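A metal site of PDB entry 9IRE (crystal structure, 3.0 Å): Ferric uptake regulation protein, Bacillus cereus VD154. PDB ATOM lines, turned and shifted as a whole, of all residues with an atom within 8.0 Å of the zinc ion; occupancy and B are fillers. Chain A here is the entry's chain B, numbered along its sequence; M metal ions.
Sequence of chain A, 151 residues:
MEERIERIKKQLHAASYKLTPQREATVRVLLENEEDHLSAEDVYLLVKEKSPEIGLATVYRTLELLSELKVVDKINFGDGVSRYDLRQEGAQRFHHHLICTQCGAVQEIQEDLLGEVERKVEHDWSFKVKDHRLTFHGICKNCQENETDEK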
ATOM      1  N   GLU A  34     -12.262   1.947  -4.630  1.00  0.00           N
ATOM      2  CA  GLU A  34     -12.338   2.810  -3.441  1.00  0.00           C
ATOM      3  C   GLU A  34     -12.663   2.024  -2.176  1.00  0.00           C
ATOM      4  O   GLU A  34     -11.947   2.114  -1.182  1.00  0.00           O
ATOM      5  CB  GLU A  34     -13.380   3.921  -3.659  1.00  0.00           C
ATOM      6  CG  GLU A  34     -13.020   4.940  -4.748  1.00  0.00           C
ATOM      7  CD  GLU A  34     -14.161   5.892  -5.111  1.00  0.00           C
ATOM      8  OE1 GLU A  34     -14.615   6.630  -4.195  1.00  0.00           O
ATOM      9  OE2 GLU A  34     -14.592   5.881  -6.302  1.00  0.00           O
ATOM     10  N   GLU A  35     -13.743   1.232  -2.195  1.00  0.00           N
ATOM     11  CA  GLU A  35     -14.123   0.491  -0.996  1.00  0.00           C
ATOM     12  C   GLU A  35     -13.013  -0.455  -0.544  1.00  0.00           C
ATOM     13  O   GLU A  35     -12.767  -0.613   0.661  1.00  0.00           O
ATOM     14  CB  GLU A  35     -15.418  -0.296  -1.251  1.00  0.00           C
ATOM     15  CG  GLU A  35     -15.964  -1.011  -0.017  1.00  0.00           C
ATOM     16  CD  GLU A  35     -17.204  -1.869  -0.301  1.00  0.00           C
ATOM     17  OE1 GLU A  35     -18.324  -1.312  -0.215  1.00  0.00           O
ATOM     18  OE2 GLU A  35     -17.051  -3.090  -0.575  1.00  0.00           O
ATOM     19  N   ASP A  36     -12.338  -1.090  -1.499  1.00  0.00           N
ATOM     20  CA  ASP A  36     -11.284  -2.048  -1.223  1.00  0.00           C
ATOM     21  C   ASP A  36     -10.156  -1.393  -0.421  1.00  0.00           C
ATOM     22  O   ASP A  36      -9.894  -0.191  -0.566  1.00  0.00           O
ATOM     23  CB  ASP A  36     -10.791  -2.606  -2.565  1.00  0.00           C
ATOM     24  CG  ASP A  36     -11.966  -2.991  -3.509  1.00  0.00           C
ATOM     25  OD1 ASP A  36     -12.925  -2.165  -3.738  1.00  0.00           O
ATOM     26  OD2 ASP A  36     -11.933  -4.132  -4.048  1.00  0.00           O
ATOM     27  N   HIS A  37      -9.497  -2.170   0.455  1.00  0.00           N
ATOM     28  CA  HIS A  37      -8.406  -1.641   1.290  1.00  0.00           C
ATOM     29  C   HIS A  37      -7.095  -2.309   0.836  1.00  0.00           C
ATOM     30  O   HIS A  37      -6.709  -3.370   1.328  1.00  0.00           O
ATOM     31  CB  HIS A  37      -8.625  -1.884   2.808  1.00  0.00           C
ATOM     32  CG  HIS A  37      -9.969  -1.453   3.330  1.00  0.00           C
ATOM     33  ND1 HIS A  37     -10.167  -0.259   3.968  1.00  0.00           N
ATOM     34  CD2 HIS A  37     -11.181  -2.044   3.238  1.00  0.00           C
ATOM     35  CE1 HIS A  37     -11.438  -0.139   4.284  1.00  0.00           C
ATOM     36  NE2 HIS A  37     -12.080  -1.215   3.870  1.00  0.00           N
ATOM     37  N   PHE A  77      -4.395  -2.479  10.036  1.00  0.00           N
ATOM     38  CA  PHE A  77      -5.494  -3.064  10.795  1.00  0.00           C
ATOM     39  C   PHE A  77      -5.059  -4.248  11.631  1.00  0.00           C
ATOM     40  O   PHE A  77      -5.919  -4.939  12.178  1.00  0.00           O
ATOM     41  CB  PHE A  77      -6.618  -3.556   9.900  1.00  0.00           C
ATOM     42  CG  PHE A  77      -7.196  -2.522   9.041  1.00  0.00           C
ATOM     43  CD1 PHE A  77      -8.107  -1.607   9.542  1.00  0.00           C
ATOM     44  CD2 PHE A  77      -6.881  -2.494   7.693  1.00  0.00           C
ATOM     45  CE1 PHE A  77      -8.657  -0.649   8.730  1.00  0.00           C
ATOM     46  CE2 PHE A  77      -7.425  -1.561   6.898  1.00  0.00           C
ATOM     47  CZ  PHE A  77      -8.322  -0.620   7.420  1.00  0.00           C
ATOM     48  N   ASP A  85      -5.650   3.131   1.758  1.00  0.00           N
ATOM     49  CA  ASP A  85      -7.046   3.402   1.501  1.00  0.00           C
ATOM     50  C   ASP A  85      -7.176   4.881   1.209  1.00  0.00           C
ATOM     51  O   ASP A  85      -6.622   5.715   1.937  1.00  0.00           O
ATOM     52  CB  ASP A  85      -7.853   2.993   2.740  1.00  0.00           C
ATOM     53  CG  ASP A  85      -9.298   3.378   2.661  1.00  0.00           C
ATOM     54  OD1 ASP A  85     -10.049   2.610   2.019  1.00  0.00           O
ATOM     55  OD2 ASP A  85      -9.676   4.427   3.253  1.00  0.00           O
ATOM     56  N   PHE A  94     -18.045   4.416  11.656  1.00  0.00           N
ATOM     57  CA  PHE A  94     -17.294   3.682  10.664  1.00  0.00           C
ATOM     58  C   PHE A  94     -17.574   2.189  10.796  1.00  0.00           C
ATOM     59  O   PHE A  94     -17.760   1.660  11.903  1.00  0.00           O
ATOM     60  CB  PHE A  94     -15.792   3.974  10.817  1.00  0.00           C
ATOM     61  CG  PHE A  94     -14.941   3.259   9.809  1.00  0.00           C
ATOM     62  CD1 PHE A  94     -14.657   3.834   8.587  1.00  0.00           C
ATOM     63  CD2 PHE A  94     -14.412   1.999  10.094  1.00  0.00           C
ATOM     64  CE1 PHE A  94     -13.861   3.174   7.677  1.00  0.00           C
ATOM     65  CE2 PHE A  94     -13.630   1.334   9.177  1.00  0.00           C
ATOM     66  CZ  PHE A  94     -13.339   1.916   7.975  1.00  0.00           C
ATOM     67  N   HIS A  95     -17.559   1.495   9.650  1.00  0.00           N
ATOM     68  CA  HIS A  95     -17.939   0.083   9.555  1.00  0.00           C
ATOM     69  C   HIS A  95     -16.877  -0.814  10.196  1.00  0.00           C
ATOM     70  O   HIS A  95     -15.922  -0.376  10.861  1.00  0.00           O
ATOM     71  CB  HIS A  95     -18.143  -0.313   8.098  1.00  0.00           C
ATOM     72  CG  HIS A  95     -16.940  -0.078   7.235  1.00  0.00           C
ATOM     73  ND1 HIS A  95     -16.766   1.072   6.505  1.00  0.00           N
ATOM     74  CD2 HIS A  95     -15.824  -0.819   7.034  1.00  0.00           C
ATOM     75  CE1 HIS A  95     -15.614   1.035   5.874  1.00  0.00           C
ATOM     76  NE2 HIS A  95     -15.021  -0.111   6.172  1.00  0.00           N
ATOM     77  N   HIS A  96     -17.078  -2.115  10.010  1.00  0.00           N
ATOM     78  CA  HIS A  96     -16.194  -3.132  10.526  1.00  0.00           C
ATOM     79  C   HIS A  96     -15.536  -3.854   9.348  1.00  0.00           C
ATOM     80  O   HIS A  96     -15.866  -3.647   8.175  1.00  0.00           O
ATOM     81  CB  HIS A  96     -16.986  -4.052  11.472  1.00  0.00           C
ATOM     82  CG  HIS A  96     -17.966  -3.315  12.364  1.00  0.00           C
ATOM     83  ND1 HIS A  96     -17.801  -1.991  12.735  1.00  0.00           N
ATOM     84  CD2 HIS A  96     -19.130  -3.718  12.943  1.00  0.00           C
ATOM     85  CE1 HIS A  96     -18.817  -1.617  13.496  1.00  0.00           C
ATOM     86  NE2 HIS A  96     -19.636  -2.639  13.635  1.00  0.00           N
ATOM     87  N   HIS A  97     -14.532  -4.669   9.661  1.00  0.00           N
ATOM     88  CA  HIS A  97     -13.743  -5.396   8.683  1.00  0.00           C
ATOM     89  C   HIS A  97     -13.495  -6.802   9.189  1.00  0.00           C
ATOM     90  O   HIS A  97     -13.149  -6.994  10.360  1.00  0.00           O
ATOM     91  CB  HIS A  97     -12.337  -4.805   8.493  1.00  0.00           C
ATOM     92  CG  HIS A  97     -12.277  -3.498   7.784  1.00  0.00           C
ATOM     93  ND1 HIS A  97     -11.912  -2.347   8.434  1.00  0.00           N
ATOM     94  CD2 HIS A  97     -12.386  -3.192   6.479  1.00  0.00           C
ATOM     95  CE1 HIS A  97     -11.835  -1.357   7.569  1.00  0.00           C
ATOM     96  NE2 HIS A  97     -12.147  -1.836   6.378  1.00  0.00           N
ATOM     97  N   LEU A  98     -13.584  -7.783   8.303  1.00  0.00           N
ATOM     98  CA  LEU A  98     -12.991  -9.085   8.551  1.00  0.00           C
ATOM     99  C   LEU A  98     -11.852  -9.224   7.551  1.00  0.00           C
ATOM    100  O   LEU A  98     -12.068  -9.109   6.355  1.00  0.00           O
ATOM    101  CB  LEU A  98     -14.048 -10.197   8.406  1.00  0.00           C
ATOM    102  CG  LEU A  98     -15.113 -10.495   9.492  1.00  0.00           C
ATOM    103  CD1 LEU A  98     -15.764  -9.301  10.185  1.00  0.00           C
ATOM    104  CD2 LEU A  98     -16.219 -11.351   8.896  1.00  0.00           C
ATOM    105  N   ILE A  99     -10.626  -9.415   8.034  1.00  0.00           N
ATOM    106  CA  ILE A  99      -9.477  -9.435   7.128  1.00  0.00           C
ATOM    107  C   ILE A  99      -8.801 -10.775   7.325  1.00  0.00           C
ATOM    108  O   ILE A  99      -8.199 -11.019   8.371  1.00  0.00           O
ATOM    109  CB  ILE A  99      -8.495  -8.279   7.354  1.00  0.00           C
ATOM    110  CG1 ILE A  99      -9.165  -6.946   7.053  1.00  0.00           C
ATOM    111  CG2 ILE A  99      -7.254  -8.450   6.464  1.00  0.00           C
ATOM    112  CD1 ILE A  99      -8.332  -5.753   7.374  1.00  0.00           C
ATOM    113  N   VAL A 106     -10.981  -9.368   2.406  1.00  0.00           N
ATOM    114  CA  VAL A 106     -11.672  -8.356   3.196  1.00  0.00           C
ATOM    115  C   VAL A 106     -13.178  -8.565   3.085  1.00  0.00           C
ATOM    116  O   VAL A 106     -13.696  -8.946   2.027  1.00  0.00           O
ATOM    117  CB  VAL A 106     -11.239  -6.962   2.705  1.00  0.00           C
ATOM    118  CG1 VAL A 106     -11.954  -5.833   3.453  1.00  0.00           C
ATOM    119  CG2 VAL A 106      -9.715  -6.824   2.814  1.00  0.00           C
ATOM    120  N   GLN A 107     -13.904  -8.324   4.174  1.00  0.00           N
ATOM    121  CA  GLN A 107     -15.376  -8.273   4.150  1.00  0.00           C
ATOM    122  C   GLN A 107     -15.835  -7.162   5.094  1.00  0.00           C
ATOM    123  O   GLN A 107     -15.550  -7.206   6.296  1.00  0.00           O
ATOM    124  CB  GLN A 107     -15.998  -9.595   4.563  1.00  0.00           C
ATOM    125  CG  GLN A 107     -15.361 -10.763   3.866  1.00  0.00           C
ATOM    126  CD  GLN A 107     -15.120 -11.934   4.782  1.00  0.00           C
ATOM    127  OE1 GLN A 107     -15.860 -12.149   5.745  1.00  0.00           O
ATOM    128  NE2 GLN A 107     -14.076 -12.696   4.490  1.00  0.00           N
ATOM    129  N   GLU A 108     -16.537  -6.178   4.570  1.00  0.00           N
ATOM    130  CA  GLU A 108     -17.119  -5.145   5.424  1.00  0.00           C
ATOM    131  C   GLU A 108     -18.414  -5.642   6.047  1.00  0.00           C
ATOM    132  O   GLU A 108     -19.181  -6.396   5.451  1.00  0.00           O
ATOM    133  CB  GLU A 108     -17.363  -3.852   4.637  1.00  0.00           C
ATOM    134  CG  GLU A 108     -16.106  -3.157   4.119  1.00  0.00           C
ATOM    135  CD  GLU A 108     -16.414  -1.798   3.516  1.00  0.00           C
ATOM    136  OE1 GLU A 108     -17.593  -1.566   3.132  1.00  0.00           O
ATOM    137  OE2 GLU A 108     -15.493  -0.953   3.428  1.00  0.00           O
ATOM    138  N   ILE A 109     -18.667  -5.228   7.284  1.00  0.00           N
ATOM    139  CA  ILE A 109     -19.924  -5.517   7.946  1.00  0.00           C
ATOM    140  C   ILE A 109     -20.749  -4.240   7.902  1.00  0.00           C
ATOM    141  O   ILE A 109     -20.342  -3.215   8.456  1.00  0.00           O
ATOM    142  CB  ILE A 109     -19.730  -5.969   9.411  1.00  0.00           C
ATOM    143  CG1 ILE A 109     -18.668  -7.061   9.546  1.00  0.00           C
ATOM    144  CG2 ILE A 109     -21.050  -6.423  10.003  1.00  0.00           C
ATOM    145  CD1 ILE A 109     -18.987  -8.309   8.814  1.00  0.00           C
ATOM    146  N   ARG A 133     -13.912   1.949  15.038  1.00  0.00           N
ATOM    147  CA  ARG A 133     -13.308   1.199  13.949  1.00  0.00           C
ATOM    148  C   ARG A 133     -12.831  -0.160  14.437  1.00  0.00           C
ATOM    149  O   ARG A 133     -11.774  -0.257  15.077  1.00  0.00           O
ATOM    150  CB  ARG A 133     -12.157   1.991  13.339  1.00  0.00           C
ATOM    151  CG  ARG A 133     -11.649   1.363  12.027  1.00  0.00           C
ATOM    152  CD  ARG A 133     -10.821   2.337  11.203  1.00  0.00           C
ATOM    153  NE  ARG A 133      -9.572   2.680  11.873  1.00  0.00           N
ATOM    154  CZ  ARG A 133      -8.796   3.708  11.537  1.00  0.00           C
ATOM    155  NH1 ARG A 133      -9.123   4.541  10.565  1.00  0.00           N
ATOM    156  NH2 ARG A 133      -7.670   3.914  12.212  1.00  0.00           N
ATOM    157  N   LEU A 134     -13.534  -1.236  14.035  1.00  0.00           N
ATOM    158  CA  LEU A 134     -13.185  -2.601  14.496  1.00  0.00           C
ATOM    159  C   LEU A 134     -12.707  -3.471  13.323  1.00  0.00           C
ATOM    160  O   LEU A 134     -13.320  -3.402  12.257  1.00  0.00           O
ATOM    161  CB  LEU A 134     -14.410  -3.231  15.150  1.00  0.00           C
ATOM    162  CG  LEU A 134     -14.364  -4.750  15.371  1.00  0.00           C
ATOM    163  CD1 LEU A 134     -13.374  -5.094  16.464  1.00  0.00           C
ATOM    164  CD2 LEU A 134     -15.747  -5.263  15.731  1.00  0.00           C
ATOM    165  N   THR A 135     -11.638  -4.251  13.536  1.00  0.00           N
ATOM    166  CA  THR A 135     -11.132  -5.160  12.497  1.00  0.00           C
ATOM    167  C   THR A 135     -10.912  -6.529  13.104  1.00  0.00           C
ATOM    168  O   THR A 135     -10.354  -6.591  14.201  1.00  0.00           O
ATOM    169  CB  THR A 135      -9.829  -4.616  11.930  1.00  0.00           C
ATOM    170  OG1 THR A 135     -10.221  -3.455  11.216  1.00  0.00           O
ATOM    171  CG2 THR A 135      -9.167  -5.608  10.984  1.00  0.00           C
HETATM  172 ZN    ZN M   1     -13.652  -1.435   4.938  1.00  0.00          ZN
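O of Glu 35 lies close to NE2 of His 37.
ND1 of His 37 is in hydrogen-bond range of OD1 of Asp 85.
A ring nitrogen (ND1) of His 97 lies within hydrogen-bond range of the side-chain hydroxyl (OG1) of Thr 135, at 3.4 Å.
O of Leu 134 sits at hydrogen-bond distance from N of His 97 (3.1 Å).
Within 4 Å of the zinc ion: His 37, His 95, His 97 and Glu 108.
The nearest printed residue that does not touch the zinc ion is Glu 35 (4.4 Å).
The zinc ion is bound by a ring nitrogen (NE2) of His 37 (1.9 Å), a ring nitrogen (NE2) of His 97 (2.1 Å), a ring nitrogen (NE2) of His 95 (2.3 Å) and the side-chain carboxylate of Glu 108 (2.4 Å).
The zinc ion has four donor atoms within binding distance.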
